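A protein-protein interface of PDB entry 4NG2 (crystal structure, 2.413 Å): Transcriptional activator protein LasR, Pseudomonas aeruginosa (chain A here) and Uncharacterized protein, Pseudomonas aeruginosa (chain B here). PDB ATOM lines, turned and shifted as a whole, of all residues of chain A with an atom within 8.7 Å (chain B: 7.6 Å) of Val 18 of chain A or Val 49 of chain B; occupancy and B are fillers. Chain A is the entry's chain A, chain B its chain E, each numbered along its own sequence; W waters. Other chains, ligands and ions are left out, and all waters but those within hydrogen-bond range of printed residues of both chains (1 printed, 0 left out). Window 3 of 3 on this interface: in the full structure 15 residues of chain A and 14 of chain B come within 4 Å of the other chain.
Water W1 lies within hydrogen-bond range of O of Pro 48 of chain B (2.9 Å), N of Ala 16 of chain A (3.2 Å) and N of Leu 17 of chain A (3.3 Å).
The indole nitrogen (NE1) of Trp 47 of chain B sits at hydrogen-bond distance from the backbone carbonyl oxygen (O) of Met 89 of chain B. O of Leu 30 of chain B sits at hydrogen-bond distance from N of Trp 47 of chain B, at 3.0 Å.
Val 18 of chain A touches two residues of chain B. Leu 22 of chain A touches none of the printed residues of chain B. Met 40 of chain A touches none of the printed residues of chain B. Of the printed residues of chain B, Thr 164 of chain A touches Leu 46, Trp 47 and Pro 48. Printed residues of chain B within 4 Å of Met 167 of chain A: Trp 47, Pro 48 and Met 89. Of the printed residues of chain A, Leu 46 of chain B touches Thr 164. Of the printed residues of chain A, Trp 47 of chain B touches Thr 164 (3.9 Å) and Met 167 (3.7 Å). Of chain A, only Val 18, Thr 164 and Met 167 come within 4 Å of Pro 48 of chain B. Of the printed residues of chain A, Met 89 of chain B touches Met 167. The nearest residue of chain A that does not touch Val 49 of chain B is Leu 17 of chain A (6.2 Å). The nearest printed residue of chain A that does not touch Trp 47 of chain B is Leu 17 of chain A (4.8 Å).
Of the 16 printed residues of chain B, 5 touch a printed residue of chain A. Printed residues of chain B that touch a printed residue of chain A: Leu 46, Trp 47, Pro 48, Val 49 and Met 89. Hydrophobic or aromatic side chains of chain A that line the printed part of chain B: Val 18 and Met 167. Among the printed residues, no Asp or Glu carboxylate lies within 4 Å of a Lys or Arg side-chain nitrogen of the other chain.
The side-chain sulfur (SD) of Met 89 of chain B sits close to the side-chain sulfur (SD) of Met 167 of chain A, 3.7 Å away. The backbone carbonyl oxygen (O) of Leu 46 of chain B sits at hydrogen-bond distance from the side-chain hydroxyl (OG1) of Thr 164 of chain A (2.6 Å).
Val 18 of chain A touches Pro 48 of chain B. Val 18 of chain A touches Val 49 of chain B (CG2 to CG1, 3.5 Å). Thr 164 of chain A touches Trp 47 of chain B (OG1 to CA, 3.9 Å). Thr 164 of chain A touches Pro 48 of chain B. Trp 47 of chain B touches Met 167 of chain A. SD of Met 167 of chain A touches CG of Pro 48 of chain B (3.7 Å).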
ATOM      1  N   ALA A  16       6.820 -22.093 -22.016  1.00  0.00           N
ATOM      2  CA  ALA A  16       7.296 -22.861 -20.861  1.00  0.00           C
ATOM      3  C   ALA A  16       6.311 -23.955 -20.415  1.00  0.00           C
ATOM      4  O   ALA A  16       6.652 -25.139 -20.394  1.00  0.00           O
ATOM      5  CB  ALA A  16       7.611 -21.940 -19.712  1.00  0.00           C
ATOM      6  N   LEU A  17       5.101 -23.550 -20.031  1.00  0.00           N
ATOM      7  CA  LEU A  17       3.995 -24.479 -19.808  1.00  0.00           C
ATOM      8  C   LEU A  17       3.428 -24.987 -21.142  1.00  0.00           C
ATOM      9  O   LEU A  17       3.069 -26.171 -21.267  1.00  0.00           O
ATOM     10  CB  LEU A  17       2.876 -23.774 -19.050  1.00  0.00           C
ATOM     11  CG  LEU A  17       3.269 -23.143 -17.721  1.00  0.00           C
ATOM     12  CD1 LEU A  17       2.351 -22.004 -17.355  1.00  0.00           C
ATOM     13  CD2 LEU A  17       3.222 -24.230 -16.698  1.00  0.00           C
ATOM     14  N   VAL A  18       3.334 -24.092 -22.132  1.00  0.00           N
ATOM     15  CA  VAL A  18       2.852 -24.482 -23.453  1.00  0.00           C
ATOM     16  C   VAL A  18       3.772 -25.536 -24.046  1.00  0.00           C
ATOM     17  O   VAL A  18       3.305 -26.489 -24.670  1.00  0.00           O
ATOM     18  CB  VAL A  18       2.741 -23.298 -24.434  1.00  0.00           C
ATOM     19  CG1 VAL A  18       2.204 -23.784 -25.778  1.00  0.00           C
ATOM     20  CG2 VAL A  18       1.832 -22.212 -23.867  1.00  0.00           C
ATOM     21  N   ASP A  19       5.076 -25.369 -23.836  1.00  0.00           N
ATOM     22  CA  ASP A  19       6.054 -26.354 -24.302  1.00  0.00           C
ATOM     23  C   ASP A  19       5.906 -27.713 -23.604  1.00  0.00           C
ATOM     24  O   ASP A  19       6.144 -28.751 -24.215  1.00  0.00           O
ATOM     25  CB  ASP A  19       7.486 -25.831 -24.145  1.00  0.00           C
ATOM     26  CG  ASP A  19       7.813 -24.723 -25.127  1.00  0.00           C
ATOM     27  OD1 ASP A  19       7.153 -24.643 -26.199  1.00  0.00           O
ATOM     28  OD2 ASP A  19       8.737 -23.930 -24.821  1.00  0.00           O
ATOM     29  N   GLY A  20       5.505 -27.698 -22.333  1.00  0.00           N
ATOM     30  CA  GLY A  20       5.360 -28.924 -21.565  1.00  0.00           C
ATOM     31  C   GLY A  20       4.133 -29.688 -22.012  1.00  0.00           C
ATOM     32  O   GLY A  20       4.132 -30.923 -22.098  1.00  0.00           O
ATOM     33  N   PHE A  21       3.077 -28.940 -22.307  1.00  0.00           N
ATOM     34  CA  PHE A  21       1.901 -29.513 -22.936  1.00  0.00           C
ATOM     35  C   PHE A  21       2.278 -30.276 -24.226  1.00  0.00           C
ATOM     36  O   PHE A  21       1.919 -31.452 -24.390  1.00  0.00           O
ATOM     37  CB  PHE A  21       0.870 -28.417 -23.227  1.00  0.00           C
ATOM     38  CG  PHE A  21       0.247 -27.809 -21.988  1.00  0.00           C
ATOM     39  CD1 PHE A  21       0.435 -28.379 -20.742  1.00  0.00           C
ATOM     40  CD2 PHE A  21      -0.541 -26.669 -22.080  1.00  0.00           C
ATOM     41  CE1 PHE A  21      -0.144 -27.822 -19.615  1.00  0.00           C
ATOM     42  CE2 PHE A  21      -1.115 -26.114 -20.962  1.00  0.00           C
ATOM     43  CZ  PHE A  21      -0.921 -26.686 -19.729  1.00  0.00           C
ATOM     44  N   LEU A  22       3.009 -29.619 -25.129  1.00  0.00           N
ATOM     45  CA  LEU A  22       3.397 -30.252 -26.393  1.00  0.00           C
ATOM     46  C   LEU A  22       4.242 -31.498 -26.157  1.00  0.00           C
ATOM     47  O   LEU A  22       3.952 -32.537 -26.730  1.00  0.00           O
ATOM     48  CB  LEU A  22       4.112 -29.272 -27.332  1.00  0.00           C
ATOM     49  CG  LEU A  22       3.375 -27.957 -27.637  1.00  0.00           C
ATOM     50  CD1 LEU A  22       4.194 -27.059 -28.579  1.00  0.00           C
ATOM     51  CD2 LEU A  22       1.958 -28.187 -28.187  1.00  0.00           C
ATOM     52  N   GLU A  23       5.256 -31.404 -25.295  1.00  0.00           N
ATOM     53  CA  GLU A  23       6.061 -32.573 -24.929  1.00  0.00           C
ATOM     54  C   GLU A  23       5.205 -33.692 -24.367  1.00  0.00           C
ATOM     55  O   GLU A  23       5.460 -34.871 -24.636  1.00  0.00           O
ATOM     56  CB  GLU A  23       7.169 -32.225 -23.936  1.00  0.00           C
ATOM     57  CG  GLU A  23       8.338 -31.521 -24.584  1.00  0.00           C
ATOM     58  CD  GLU A  23       8.716 -32.104 -25.951  1.00  0.00           C
ATOM     59  OE1 GLU A  23       8.738 -33.358 -26.108  1.00  0.00           O
ATOM     60  OE2 GLU A  23       9.001 -31.293 -26.868  1.00  0.00           O
ATOM     61  N   LEU A  24       4.192 -33.331 -23.588  1.00  0.00           N
ATOM     62  CA  LEU A  24       3.249 -34.316 -23.076  1.00  0.00           C
ATOM     63  C   LEU A  24       2.606 -35.107 -24.234  1.00  0.00           C
ATOM     64  O   LEU A  24       2.635 -36.341 -24.267  1.00  0.00           O
ATOM     65  CB  LEU A  24       2.192 -33.613 -22.222  1.00  0.00           C
ATOM     66  CG  LEU A  24       1.791 -34.280 -20.912  1.00  0.00           C
ATOM     67  CD1 LEU A  24       2.972 -34.881 -20.165  1.00  0.00           C
ATOM     68  CD2 LEU A  24       1.082 -33.281 -20.035  1.00  0.00           C
ATOM     69  N   GLU A  25       2.060 -34.390 -25.203  1.00  0.00           N
ATOM     70  CA  GLU A  25       1.439 -35.029 -26.355  1.00  0.00           C
ATOM     71  C   GLU A  25       2.441 -35.773 -27.253  1.00  0.00           C
ATOM     72  O   GLU A  25       2.066 -36.711 -27.954  1.00  0.00           O
ATOM     73  CB  GLU A  25       0.701 -33.980 -27.176  1.00  0.00           C
ATOM     74  CG  GLU A  25      -0.266 -33.161 -26.361  1.00  0.00           C
ATOM     75  CD  GLU A  25      -1.660 -33.161 -26.963  1.00  0.00           C
ATOM     76  OE1 GLU A  25      -1.789 -32.732 -28.137  1.00  0.00           O
ATOM     77  OE2 GLU A  25      -2.617 -33.601 -26.274  1.00  0.00           O
ATOM     78  N   ARG A  26       3.710 -35.360 -27.230  1.00  0.00           N
ATOM     79  CA  ARG A  26       4.716 -35.973 -28.097  1.00  0.00           C
ATOM     80  C   ARG A  26       5.309 -37.217 -27.477  1.00  0.00           C
ATOM     81  O   ARG A  26       6.087 -37.914 -28.126  1.00  0.00           O
ATOM     82  CB  ARG A  26       5.869 -35.009 -28.430  1.00  0.00           C
ATOM     83  CG  ARG A  26       5.522 -33.829 -29.335  1.00  0.00           C
ATOM     84  CD  ARG A  26       6.741 -32.897 -29.507  1.00  0.00           C
ATOM     85  NE  ARG A  26       6.451 -31.695 -30.307  1.00  0.00           N
ATOM     86  CZ  ARG A  26       7.236 -30.617 -30.357  1.00  0.00           C
ATOM     87  NH1 ARG A  26       8.361 -30.576 -29.647  1.00  0.00           N
ATOM     88  NH2 ARG A  26       6.895 -29.577 -31.107  1.00  0.00           N
ATOM     89  N   ILE A  36       7.634 -35.911 -17.840  1.00  0.00           N
ATOM     90  CA  ILE A  36       7.130 -34.582 -18.230  1.00  0.00           C
ATOM     91  C   ILE A  36       6.029 -34.098 -17.287  1.00  0.00           C
ATOM     92  O   ILE A  36       5.971 -32.915 -16.931  1.00  0.00           O
ATOM     93  CB  ILE A  36       6.637 -34.541 -19.705  1.00  0.00           C
ATOM     94  CG1 ILE A  36       7.816 -34.745 -20.646  1.00  0.00           C
ATOM     95  CG2 ILE A  36       5.949 -33.195 -20.027  1.00  0.00           C
ATOM     96  CD1 ILE A  36       7.424 -35.216 -22.022  1.00  0.00           C
ATOM     97  N   MET A  40       6.385 -30.712 -14.987  1.00  0.00           N
ATOM     98  CA  MET A  40       5.384 -29.666 -15.116  1.00  0.00           C
ATOM     99  C   MET A  40       4.722 -29.347 -13.797  1.00  0.00           C
ATOM    100  O   MET A  40       4.386 -28.197 -13.531  1.00  0.00           O
ATOM    101  CB  MET A  40       4.312 -30.099 -16.109  1.00  0.00           C
ATOM    102  CG  MET A  40       4.789 -30.029 -17.537  1.00  0.00           C
ATOM    103  SD  MET A  40       3.681 -29.025 -18.519  1.00  0.00           S
ATOM    104  CE  MET A  40       2.618 -30.333 -19.108  1.00  0.00           C
ATOM    105  N   THR A 164      -4.819 -23.215 -15.413  1.00  0.00           N
ATOM    106  CA  THR A 164      -3.687 -23.841 -16.044  1.00  0.00           C
ATOM    107  C   THR A 164      -3.683 -25.321 -15.721  1.00  0.00           C
ATOM    108  O   THR A 164      -3.301 -26.137 -16.544  1.00  0.00           O
ATOM    109  CB  THR A 164      -2.403 -23.211 -15.550  1.00  0.00           C
ATOM    110  OG1 THR A 164      -2.347 -21.857 -16.022  1.00  0.00           O
ATOM    111  CG2 THR A 164      -1.203 -23.989 -16.051  1.00  0.00           C
ATOM    112  N   MET A 167      -6.100 -27.352 -17.750  1.00  0.00           N
ATOM    113  CA  MET A 167      -5.560 -27.637 -19.071  1.00  0.00           C
ATOM    114  C   MET A 167      -4.520 -28.745 -19.001  1.00  0.00           C
ATOM    115  O   MET A 167      -4.411 -29.572 -19.923  1.00  0.00           O
ATOM    116  CB  MET A 167      -4.966 -26.388 -19.697  1.00  0.00           C
ATOM    117  CG  MET A 167      -5.999 -25.364 -19.996  1.00  0.00           C
ATOM    118  SD  MET A 167      -5.283 -23.952 -20.835  1.00  0.00           S
ATOM    119  CE  MET A 167      -6.697 -22.857 -20.738  1.00  0.00           C
ATOM    120  N   TYR A 171      -4.624 -32.193 -21.214  1.00  0.00           N
ATOM    121  CA  TYR A 171      -3.542 -32.760 -22.021  1.00  0.00           C
ATOM    122  C   TYR A 171      -3.081 -34.092 -21.462  1.00  0.00           C
ATOM    123  O   TYR A 171      -2.628 -34.973 -22.202  1.00  0.00           O
ATOM    124  CB  TYR A 171      -2.351 -31.803 -22.093  1.00  0.00           C
ATOM    125  CG  TYR A 171      -2.519 -30.680 -23.094  1.00  0.00           C
ATOM    126  CD1 TYR A 171      -2.173 -30.857 -24.421  1.00  0.00           C
ATOM    127  CD2 TYR A 171      -3.013 -29.438 -22.705  1.00  0.00           C
ATOM    128  CE1 TYR A 171      -2.315 -29.830 -25.345  1.00  0.00           C
ATOM    129  CE2 TYR A 171      -3.166 -28.400 -23.621  1.00  0.00           C
ATOM    130  CZ  TYR A 171      -2.814 -28.612 -24.939  1.00  0.00           C
ATOM    131  OH  TYR A 171      -2.955 -27.610 -25.854  1.00  0.00           O
ATOM    132  N   ASP B  29       4.237 -12.365 -16.364  1.00  0.00           N
ATOM    133  CA  ASP B  29       3.591 -11.965 -17.610  1.00  0.00           C
ATOM    134  C   ASP B  29       2.309 -12.743 -17.942  1.00  0.00           C
ATOM    135  O   ASP B  29       1.363 -12.193 -18.527  1.00  0.00           O
ATOM    136  CB  ASP B  29       4.597 -12.129 -18.748  1.00  0.00           C
ATOM    137  CG  ASP B  29       5.886 -11.350 -18.508  1.00  0.00           C
ATOM    138  OD1 ASP B  29       5.849 -10.312 -17.800  1.00  0.00           O
ATOM    139  OD2 ASP B  29       6.937 -11.779 -19.033  1.00  0.00           O
ATOM    140  N   LEU B  30       2.292 -14.019 -17.561  1.00  0.00           N
ATOM    141  CA  LEU B  30       1.205 -14.930 -17.890  1.00  0.00           C
ATOM    142  C   LEU B  30       0.013 -14.802 -16.963  1.00  0.00           C
ATOM    143  O   LEU B  30      -1.000 -15.471 -17.169  1.00  0.00           O
ATOM    144  CB  LEU B  30       1.710 -16.365 -17.871  1.00  0.00           C
ATOM    145  CG  LEU B  30       2.866 -16.609 -18.840  1.00  0.00           C
ATOM    146  CD1 LEU B  30       3.475 -18.000 -18.652  1.00  0.00           C
ATOM    147  CD2 LEU B  30       2.371 -16.406 -20.271  1.00  0.00           C
ATOM    148  N   MET B  31       0.120 -13.937 -15.955  1.00  0.00           N
ATOM    149  CA  MET B  31      -1.008 -13.662 -15.054  1.00  0.00           C
ATOM    150  C   MET B  31      -2.030 -12.688 -15.677  1.00  0.00           C
ATOM    151  O   MET B  31      -1.660 -11.763 -16.389  1.00  0.00           O
ATOM    152  CB  MET B  31      -0.509 -13.121 -13.702  1.00  0.00           C
ATOM    153  CG  MET B  31       0.322 -14.104 -12.866  1.00  0.00           C
ATOM    154  SD  MET B  31      -0.591 -15.520 -12.191  1.00  0.00           S
ATOM    155  CE  MET B  31      -1.796 -14.782 -11.090  1.00  0.00           C
ATOM    156  N   VAL B  32      -3.312 -12.899 -15.394  1.00  0.00           N
ATOM    157  CA  VAL B  32      -4.365 -12.081 -15.958  1.00  0.00           C
ATOM    158  C   VAL B  32      -5.404 -11.759 -14.884  1.00  0.00           C
ATOM    159  O   VAL B  32      -5.599 -12.542 -13.951  1.00  0.00           O
ATOM    160  CB  VAL B  32      -5.057 -12.785 -17.164  1.00  0.00           C
ATOM    161  CG1 VAL B  32      -4.056 -13.030 -18.310  1.00  0.00           C
ATOM    162  CG2 VAL B  32      -5.732 -14.090 -16.722  1.00  0.00           C
ATOM    163  N   LEU B  45      -5.467 -14.965 -12.048  1.00  0.00           N
ATOM    164  CA  LEU B  45      -5.499 -16.272 -12.701  1.00  0.00           C
ATOM    165  C   LEU B  45      -4.272 -16.441 -13.564  1.00  0.00           C
ATOM    166  O   LEU B  45      -3.953 -15.557 -14.341  1.00  0.00           O
ATOM    167  CB  LEU B  45      -6.734 -16.341 -13.600  1.00  0.00           C
ATOM    168  CG  LEU B  45      -7.973 -17.172 -13.268  1.00  0.00           C
ATOM    169  CD1 LEU B  45      -8.076 -17.500 -11.803  1.00  0.00           C
ATOM    170  CD2 LEU B  45      -9.258 -16.496 -13.807  1.00  0.00           C
ATOM    171  N   LEU B  46      -3.582 -17.567 -13.432  1.00  0.00           N
ATOM    172  CA  LEU B  46      -2.408 -17.851 -14.259  1.00  0.00           C
ATOM    173  C   LEU B  46      -2.820 -18.554 -15.537  1.00  0.00           C
ATOM    174  O   LEU B  46      -3.525 -19.554 -15.480  1.00  0.00           O
ATOM    175  CB  LEU B  46      -1.438 -18.751 -13.507  1.00  0.00           C
ATOM    176  CG  LEU B  46      -0.528 -19.579 -14.399  1.00  0.00           C
ATOM    177  CD1 LEU B  46       0.571 -18.712 -14.938  1.00  0.00           C
ATOM    178  CD2 LEU B  46       0.056 -20.727 -13.606  1.00  0.00           C
ATOM    179  N   TRP B  47      -2.379 -18.033 -16.682  1.00  0.00           N
ATOM    180  CA  TRP B  47      -2.748 -18.575 -17.995  1.00  0.00           C
ATOM    181  C   TRP B  47      -1.493 -18.980 -18.748  1.00  0.00           C
ATOM    182  O   TRP B  47      -0.463 -18.326 -18.624  1.00  0.00           O
ATOM    183  CB  TRP B  47      -3.520 -17.549 -18.814  1.00  0.00           C
ATOM    184  CG  TRP B  47      -4.638 -18.128 -19.607  1.00  0.00           C
ATOM    185  CD1 TRP B  47      -4.637 -18.432 -20.946  1.00  0.00           C
ATOM    186  CD2 TRP B  47      -5.935 -18.468 -19.121  1.00  0.00           C
ATOM    187  NE1 TRP B  47      -5.850 -18.950 -21.311  1.00  0.00           N
ATOM    188  CE2 TRP B  47      -6.671 -18.976 -20.212  1.00  0.00           C
ATOM    189  CE3 TRP B  47      -6.549 -18.399 -17.867  1.00  0.00           C
ATOM    190  CZ2 TRP B  47      -7.987 -19.422 -20.080  1.00  0.00           C
ATOM    191  CZ3 TRP B  47      -7.854 -18.836 -17.740  1.00  0.00           C
ATOM    192  CH2 TRP B  47      -8.560 -19.338 -18.835  1.00  0.00           C
ATOM    193  N   PRO B  48      -1.572 -20.076 -19.514  1.00  0.00           N
ATOM    194  CA  PRO B  48      -0.402 -20.618 -20.209  1.00  0.00           C
ATOM    195  C   PRO B  48       0.164 -19.666 -21.251  1.00  0.00           C
ATOM    196  O   PRO B  48       1.324 -19.817 -21.636  1.00  0.00           O
ATOM    197  CB  PRO B  48      -0.946 -21.883 -20.888  1.00  0.00           C
ATOM    198  CG  PRO B  48      -2.112 -22.286 -20.024  1.00  0.00           C
ATOM    199  CD  PRO B  48      -2.730 -20.981 -19.586  1.00  0.00           C
ATOM    200  N   VAL B  49      -0.649 -18.727 -21.719  1.00  0.00           N
ATOM    201  CA  VAL B  49      -0.175 -17.735 -22.662  1.00  0.00           C
ATOM    202  C   VAL B  49      -0.736 -16.393 -22.259  1.00  0.00           C
ATOM    203  O   VAL B  49      -1.726 -16.340 -21.528  1.00  0.00           O
ATOM    204  CB  VAL B  49      -0.616 -18.052 -24.108  1.00  0.00           C
ATOM    205  CG1 VAL B  49      -0.312 -19.494 -24.446  1.00  0.00           C
ATOM    206  CG2 VAL B  49      -2.087 -17.760 -24.292  1.00  0.00           C
ATOM    207  N   PRO B  50      -0.107 -15.301 -22.730  1.00  0.00           N
ATOM    208  CA  PRO B  50      -0.682 -13.984 -22.442  1.00  0.00           C
ATOM    209  C   PRO B  50      -2.064 -13.924 -23.069  1.00  0.00           C
ATOM    210  O   PRO B  50      -2.224 -14.291 -24.234  1.00  0.00           O
ATOM    211  CB  PRO B  50       0.284 -13.010 -23.136  1.00  0.00           C
ATOM    212  CG  PRO B  50       0.983 -13.822 -24.180  1.00  0.00           C
ATOM    213  CD  PRO B  50       1.065 -15.221 -23.625  1.00  0.00           C
ATOM    214  N   ALA B  51      -3.050 -13.475 -22.303  1.00  0.00           N
ATOM    215  CA  ALA B  51      -4.427 -13.554 -22.736  1.00  0.00           C
ATOM    216  C   ALA B  51      -5.341 -12.523 -22.092  1.00  0.00           C
ATOM    217  O   ALA B  51      -6.566 -12.734 -22.045  1.00  0.00           O
ATOM    218  CB  ALA B  51      -4.970 -14.973 -22.479  1.00  0.00           C
ATOM    219  N   GLN B  52      -4.773 -11.417 -21.605  1.00  0.00           N
ATOM    220  CA  GLN B  52      -5.582 -10.347 -20.989  1.00  0.00           C
ATOM    221  C   GLN B  52      -6.714  -9.799 -21.893  1.00  0.00           C
ATOM    222  O   GLN B  52      -7.869  -9.683 -21.444  1.00  0.00           O
ATOM    223  CB  GLN B  52      -4.694  -9.210 -20.459  1.00  0.00           C
ATOM    224  CG  GLN B  52      -4.735  -9.060 -18.927  1.00  0.00           C
ATOM    225  CD  GLN B  52      -6.056  -8.499 -18.450  1.00  0.00           C
ATOM    226  OE1 GLN B  52      -6.610  -7.632 -19.105  1.00  0.00           O
ATOM    227  NE2 GLN B  52      -6.569  -8.984 -17.318  1.00  0.00           N
ATOM    228  N   THR B  87      -7.871 -18.680 -31.224  1.00  0.00           N
ATOM    229  CA  THR B  87      -7.181 -19.837 -30.619  1.00  0.00           C
ATOM    230  C   THR B  87      -7.947 -20.470 -29.447  1.00  0.00           C
ATOM    231  O   THR B  87      -8.576 -19.767 -28.646  1.00  0.00           O
ATOM    232  CB  THR B  87      -5.770 -19.456 -30.103  1.00  0.00           C
ATOM    233  OG1 THR B  87      -5.892 -18.454 -29.080  1.00  0.00           O
ATOM    234  CG2 THR B  87      -4.899 -18.910 -31.229  1.00  0.00           C
ATOM    235  N   MET B  89      -6.904 -21.369 -26.765  1.00  0.00           N
ATOM    236  CA  MET B  89      -6.445 -20.743 -25.532  1.00  0.00           C
ATOM    237  C   MET B  89      -7.151 -19.398 -25.243  1.00  0.00           C
ATOM    238  O   MET B  89      -7.399 -19.035 -24.089  1.00  0.00           O
ATOM    239  CB  MET B  89      -4.924 -20.578 -25.564  1.00  0.00           C
ATOM    240  CG  MET B  89      -4.284 -20.700 -24.213  1.00  0.00           C
ATOM    241  SD  MET B  89      -3.827 -22.382 -23.804  1.00  0.00           S
ATOM    242  CE  MET B  89      -2.310 -22.506 -24.713  1.00  0.00           C
ATOM    243  N   GLN B  90      -7.500 -18.658 -26.283  1.00  0.00           N
ATOM    244  CA  GLN B  90      -8.244 -17.441 -26.048  1.00  0.00           C
ATOM    245  C   GLN B  90      -9.697 -17.746 -25.795  1.00  0.00           C
ATOM    246  O   GLN B  90     -10.337 -17.086 -24.993  1.00  0.00           O
ATOM    247  CB  GLN B  90      -8.122 -16.498 -27.228  1.00  0.00           C
ATOM    248  CG  GLN B  90      -6.775 -15.875 -27.345  1.00  0.00           C
ATOM    249  CD  GLN B  90      -6.728 -14.976 -28.545  1.00  0.00           C
ATOM    250  OE1 GLN B  90      -6.579 -15.447 -29.685  1.00  0.00           O
ATOM    251  NE2 GLN B  90      -6.897 -13.664 -28.313  1.00  0.00           N
ATOM    252  N   ALA B  93     -10.065 -18.468 -22.284  1.00  0.00           N
ATOM    253  CA  ALA B  93      -9.873 -17.288 -21.452  1.00  0.00           C
ATOM    254  C   ALA B  93     -11.153 -16.479 -21.454  1.00  0.00           C
ATOM    255  O   ALA B  93     -11.577 -15.957 -20.420  1.00  0.00           O
ATOM    256  CB  ALA B  93      -8.710 -16.458 -21.945  1.00  0.00           C
HETATM  257  O   HOH W   1       4.052 -20.660 -21.210  1.00  0.00           O
